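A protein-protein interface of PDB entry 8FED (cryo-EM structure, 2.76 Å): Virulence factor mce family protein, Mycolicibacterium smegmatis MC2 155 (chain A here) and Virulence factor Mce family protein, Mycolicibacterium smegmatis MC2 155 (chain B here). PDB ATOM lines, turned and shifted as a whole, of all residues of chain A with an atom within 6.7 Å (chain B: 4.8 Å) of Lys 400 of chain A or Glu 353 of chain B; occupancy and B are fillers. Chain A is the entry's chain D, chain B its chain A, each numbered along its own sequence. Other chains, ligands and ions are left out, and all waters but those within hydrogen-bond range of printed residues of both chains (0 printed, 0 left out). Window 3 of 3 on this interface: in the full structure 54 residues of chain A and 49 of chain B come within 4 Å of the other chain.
O of Glu 353 of chain B is in hydrogen-bond range of NZ of Lys 400 of chain A (2.9 Å). O of Ser 398 of chain A sits close to O of Gly 351 of chain B (3.0 Å).
Among the printed residues, pairs that only touch across the chains: Ser 398 of chain A with Gly 354 of chain B, Tyr 397 of chain A with Gly 354 of chain B, Ala 396 of chain A with Trp 359 of chain B, Lys 400 of chain A with Gly 354 of chain B, Tyr 397 of chain A with Gly 351 of chain B and Tyr 397 of chain A with Glu 353 of chain B.
Printed residues of chain B within 4 Å of Ala 396 of chain A: Trp 359 (3.7 Å). Of the printed residues of chain B, Tyr 397 of chain A touches Gly 351, Glu 353 and Gly 354. Of the printed residues of chain B, Ser 398 of chain A touches Gly 351 (3.0 Å) and Gly 354 (3.3 Å). Of chain B, only Glu 353 and Gly 354 come within 4 Å of Lys 400 of chain A. Of the printed residues of chain A, Glu 353 of chain B touches Tyr 397 (3.998 Å) and Lys 400 (2.9 Å). Of the printed residues of chain A, Gly 354 of chain B touches Tyr 397, Ser 398 and Lys 400. Printed residues of chain A within 4 Å of Trp 359 of chain B: Ala 396. The nearest printed residue of chain A that does not touch Glu 353 of chain B is Ala 396 of chain A (4.6 Å). The nearest printed residue of chain B that does not touch Ala 396 of chain A is Glu 353 of chain B (4.6 Å).
Hydrophobic or aromatic side chains of chain B that line the printed part of chain A: Trp 359. Of the 9 printed residues of chain A, 4 touch a printed residue of chain B. Hydrophobic or aromatic side chains of chain A within 4 Å of the printed part of chain B: Ala 396. Among the printed residues, no Asp or Glu carboxylate lies within 4 Å of a Lys or Arg side-chain nitrogen of the other chain.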
ATOM      1  N   ALA A 396     -15.135 -15.059   9.896  1.00  0.00           N
ATOM      2  CA  ALA A 396     -16.149 -15.063  10.941  1.00  0.00           C
ATOM      3  C   ALA A 396     -17.015 -13.825  10.781  1.00  0.00           C
ATOM      4  O   ALA A 396     -16.496 -12.724  10.572  1.00  0.00           O
ATOM      5  CB  ALA A 396     -15.515 -15.094  12.333  1.00  0.00           C
ATOM      6  N   TYR A 397     -18.327 -14.001  10.881  1.00  0.00           N
ATOM      7  CA  TYR A 397     -19.282 -12.943  10.584  1.00  0.00           C
ATOM      8  C   TYR A 397     -19.699 -12.250  11.873  1.00  0.00           C
ATOM      9  O   TYR A 397     -20.024 -12.914  12.862  1.00  0.00           O
ATOM     10  CB  TYR A 397     -20.502 -13.514   9.861  1.00  0.00           C
ATOM     11  CG  TYR A 397     -20.135 -14.394   8.688  1.00  0.00           C
ATOM     12  CD1 TYR A 397     -19.715 -13.844   7.488  1.00  0.00           C
ATOM     13  CD2 TYR A 397     -20.190 -15.776   8.790  1.00  0.00           C
ATOM     14  CE1 TYR A 397     -19.369 -14.640   6.418  1.00  0.00           C
ATOM     15  CE2 TYR A 397     -19.845 -16.583   7.725  1.00  0.00           C
ATOM     16  CZ  TYR A 397     -19.435 -16.009   6.541  1.00  0.00           C
ATOM     17  OH  TYR A 397     -19.092 -16.807   5.475  1.00  0.00           O
ATOM     18  N   SER A 398     -19.679 -10.915  11.859  1.00  0.00           N
ATOM     19  CA  SER A 398     -20.025 -10.151  13.053  1.00  0.00           C
ATOM     20  C   SER A 398     -21.493 -10.306  13.426  1.00  0.00           C
ATOM     21  O   SER A 398     -21.852 -10.140  14.597  1.00  0.00           O
ATOM     22  CB  SER A 398     -19.686  -8.677  12.848  1.00  0.00           C
ATOM     23  OG  SER A 398     -19.918  -7.934  14.028  1.00  0.00           O
ATOM     24  N   GLU A 399     -22.353 -10.614  12.459  1.00  0.00           N
ATOM     25  CA  GLU A 399     -23.773 -10.810  12.704  1.00  0.00           C
ATOM     26  C   GLU A 399     -24.234 -12.087  12.021  1.00  0.00           C
ATOM     27  O   GLU A 399     -23.717 -12.470  10.968  1.00  0.00           O
ATOM     28  CB  GLU A 399     -24.605  -9.622  12.201  1.00  0.00           C
ATOM     29  CG  GLU A 399     -24.119  -8.268  12.690  1.00  0.00           C
ATOM     30  CD  GLU A 399     -24.980  -7.123  12.197  1.00  0.00           C
ATOM     31  OE1 GLU A 399     -26.208  -7.310  12.072  1.00  0.00           O
ATOM     32  OE2 GLU A 399     -24.425  -6.037  11.931  1.00  0.00           O
ATOM     33  N   LYS A 400     -25.218 -12.746  12.633  1.00  0.00           N
ATOM     34  CA  LYS A 400     -25.716 -14.013  12.110  1.00  0.00           C
ATOM     35  C   LYS A 400     -26.537 -13.852  10.839  1.00  0.00           C
ATOM     36  O   LYS A 400     -26.868 -14.862  10.209  1.00  0.00           O
ATOM     37  CB  LYS A 400     -26.552 -14.725  13.174  1.00  0.00           C
ATOM     38  CG  LYS A 400     -25.728 -15.371  14.275  1.00  0.00           C
ATOM     39  CD  LYS A 400     -26.618 -16.044  15.307  1.00  0.00           C
ATOM     40  CE  LYS A 400     -25.800 -16.819  16.324  1.00  0.00           C
ATOM     41  NZ  LYS A 400     -24.788 -15.956  16.994  1.00  0.00           N
ATOM     42  N   ARG A 401     -26.880 -12.623  10.452  1.00  0.00           N
ATOM     43  CA  ARG A 401     -27.584 -12.390   9.200  1.00  0.00           C
ATOM     44  C   ARG A 401     -26.650 -12.199   8.016  1.00  0.00           C
ATOM     45  O   ARG A 401     -27.100 -12.303   6.870  1.00  0.00           O
ATOM     46  CB  ARG A 401     -28.495 -11.165   9.322  1.00  0.00           C
ATOM     47  CG  ARG A 401     -27.749  -9.874   9.601  1.00  0.00           C
ATOM     48  CD  ARG A 401     -28.666  -8.668   9.526  1.00  0.00           C
ATOM     49  NE  ARG A 401     -27.957  -7.432   9.834  1.00  0.00           N
ATOM     50  CZ  ARG A 401     -27.257  -6.731   8.953  1.00  0.00           C
ATOM     51  NH1 ARG A 401     -27.149  -7.115   7.693  1.00  0.00           N
ATOM     52  NH2 ARG A 401     -26.648  -5.617   9.347  1.00  0.00           N
ATOM     53  N   LEU A 402     -25.369 -11.929   8.258  1.00  0.00           N
ATOM     54  CA  LEU A 402     -24.402 -11.720   7.188  1.00  0.00           C
ATOM     55  C   LEU A 402     -23.797 -13.016   6.668  1.00  0.00           C
ATOM     56  O   LEU A 402     -22.980 -12.971   5.743  1.00  0.00           O
ATOM     57  CB  LEU A 402     -23.278 -10.793   7.661  1.00  0.00           C
ATOM     58  CG  LEU A 402     -23.628  -9.325   7.895  1.00  0.00           C
ATOM     59  CD1 LEU A 402     -22.376  -8.518   8.195  1.00  0.00           C
ATOM     60  CD2 LEU A 402     -24.352  -8.760   6.691  1.00  0.00           C
ATOM     61  N   GLN A 403     -24.165 -14.157   7.235  1.00  0.00           N
ATOM     62  CA  GLN A 403     -23.620 -15.431   6.785  1.00  0.00           C
ATOM     63  C   GLN A 403     -24.345 -15.887   5.523  1.00  0.00           C
ATOM     64  O   GLN A 403     -25.568 -16.057   5.554  1.00  0.00           O
ATOM     65  CB  GLN A 403     -23.758 -16.482   7.876  1.00  0.00           C
ATOM     66  CG  GLN A 403     -23.188 -17.837   7.506  1.00  0.00           C
ATOM     67  CD  GLN A 403     -23.463 -18.888   8.558  1.00  0.00           C
ATOM     68  OE1 GLN A 403     -23.949 -18.581   9.646  1.00  0.00           O
ATOM     69  NE2 GLN A 403     -23.158 -20.139   8.239  1.00  0.00           N
ATOM     70  N   TRP A 417     -24.344 -10.963  -1.531  1.00  0.00           N
ATOM     71  CA  TRP A 417     -23.879 -12.333  -1.706  1.00  0.00           C
ATOM     72  C   TRP A 417     -23.968 -12.723  -3.174  1.00  0.00           C
ATOM     73  O   TRP A 417     -25.060 -12.727  -3.751  1.00  0.00           O
ATOM     74  CB  TRP A 417     -24.703 -13.286  -0.844  1.00  0.00           C
ATOM     75  CG  TRP A 417     -24.726 -12.896   0.595  1.00  0.00           C
ATOM     76  CD1 TRP A 417     -23.772 -12.192   1.268  1.00  0.00           C
ATOM     77  CD2 TRP A 417     -25.771 -13.154   1.536  1.00  0.00           C
ATOM     78  NE1 TRP A 417     -24.146 -12.015   2.574  1.00  0.00           N
ATOM     79  CE2 TRP A 417     -25.374 -12.594   2.763  1.00  0.00           C
ATOM     80  CE3 TRP A 417     -27.001 -13.810   1.462  1.00  0.00           C
ATOM     81  CZ2 TRP A 417     -26.158 -12.677   3.907  1.00  0.00           C
ATOM     82  CZ3 TRP A 417     -27.781 -13.888   2.598  1.00  0.00           C
ATOM     83  CH2 TRP A 417     -27.357 -13.324   3.804  1.00  0.00           C
ATOM     84  N   GLY B 351     -20.331  -8.668  17.534  1.00  0.00           N
ATOM     85  CA  GLY B 351     -18.943  -9.037  17.664  1.00  0.00           C
ATOM     86  C   GLY B 351     -18.684 -10.412  17.089  1.00  0.00           C
ATOM     87  O   GLY B 351     -19.463 -10.919  16.277  1.00  0.00           O
ATOM     88  N   PRO B 352     -17.570 -11.033  17.479  1.00  0.00           N
ATOM     89  CA  PRO B 352     -17.254 -12.374  16.970  1.00  0.00           C
ATOM     90  C   PRO B 352     -18.341 -13.377  17.323  1.00  0.00           C
ATOM     91  O   PRO B 352     -18.899 -13.354  18.420  1.00  0.00           O
ATOM     92  CB  PRO B 352     -15.928 -12.713  17.660  1.00  0.00           C
ATOM     93  CG  PRO B 352     -15.817 -11.758  18.796  1.00  0.00           C
ATOM     94  CD  PRO B 352     -16.508 -10.515  18.354  1.00  0.00           C
ATOM     95  N   GLU B 353     -18.642 -14.257  16.365  1.00  0.00           N
ATOM     96  CA  GLU B 353     -19.666 -15.295  16.487  1.00  0.00           C
ATOM     97  C   GLU B 353     -21.067 -14.720  16.678  1.00  0.00           C
ATOM     98  O   GLU B 353     -21.968 -15.424  17.144  1.00  0.00           O
ATOM     99  CB  GLU B 353     -19.340 -16.281  17.616  1.00  0.00           C
ATOM    100  CG  GLU B 353     -18.002 -16.975  17.456  1.00  0.00           C
ATOM    101  CD  GLU B 353     -17.947 -17.859  16.228  1.00  0.00           C
ATOM    102  OE1 GLU B 353     -18.991 -18.438  15.860  1.00  0.00           O
ATOM    103  OE2 GLU B 353     -16.857 -17.977  15.630  1.00  0.00           O
ATOM    104  N   GLY B 354     -21.274 -13.455  16.323  1.00  0.00           N
ATOM    105  CA  GLY B 354     -22.577 -12.832  16.362  1.00  0.00           C
ATOM    106  C   GLY B 354     -22.841 -11.971  17.581  1.00  0.00           C
ATOM    107  O   GLY B 354     -23.767 -11.154  17.550  1.00  0.00           O
ATOM    108  N   ARG B 355     -22.059 -12.126  18.644  1.00  0.00           N
ATOM    109  CA  ARG B 355     -22.245 -11.378  19.876  1.00  0.00           C
ATOM    110  C   ARG B 355     -20.940 -10.699  20.262  1.00  0.00           C
ATOM    111  O   ARG B 355     -19.862 -11.196  19.927  1.00  0.00           O
ATOM    112  CB  ARG B 355     -22.708 -12.302  21.014  1.00  0.00           C
ATOM    113  CG  ARG B 355     -23.893 -13.188  20.662  1.00  0.00           C
ATOM    114  CD  ARG B 355     -24.325 -14.064  21.834  1.00  0.00           C
ATOM    115  NE  ARG B 355     -23.248 -14.908  22.342  1.00  0.00           N
ATOM    116  CZ  ARG B 355     -22.575 -14.676  23.461  1.00  0.00           C
ATOM    117  NH1 ARG B 355     -22.839 -13.626  24.222  1.00  0.00           N
ATOM    118  NH2 ARG B 355     -21.612 -15.518  23.827  1.00  0.00           N
ATOM    119  N   TRP B 359     -11.637 -12.316  20.748  1.00  0.00           N
ATOM    120  CA  TRP B 359     -10.988 -13.594  20.521  1.00  0.00           C
ATOM    121  C   TRP B 359     -10.045 -13.904  21.680  1.00  0.00           C
ATOM    122  O   TRP B 359      -9.599 -13.011  22.406  1.00  0.00           O
ATOM    123  CB  TRP B 359     -10.193 -13.585  19.212  1.00  0.00           C
ATOM    124  CG  TRP B 359     -10.987 -13.261  17.982  1.00  0.00           C
ATOM    125  CD1 TRP B 359     -10.875 -12.143  17.209  1.00  0.00           C
ATOM    126  CD2 TRP B 359     -12.005 -14.066  17.375  1.00  0.00           C
ATOM    127  NE1 TRP B 359     -11.760 -12.199  16.164  1.00  0.00           N
ATOM    128  CE2 TRP B 359     -12.467 -13.370  16.243  1.00  0.00           C
ATOM    129  CE3 TRP B 359     -12.572 -15.305  17.682  1.00  0.00           C
ATOM    130  CZ2 TRP B 359     -13.467 -13.872  15.417  1.00  0.00           C
ATOM    131  CZ3 TRP B 359     -13.567 -15.801  16.861  1.00  0.00           C
ATOM    132  CH2 TRP B 359     -14.002 -15.086  15.743  1.00  0.00           C
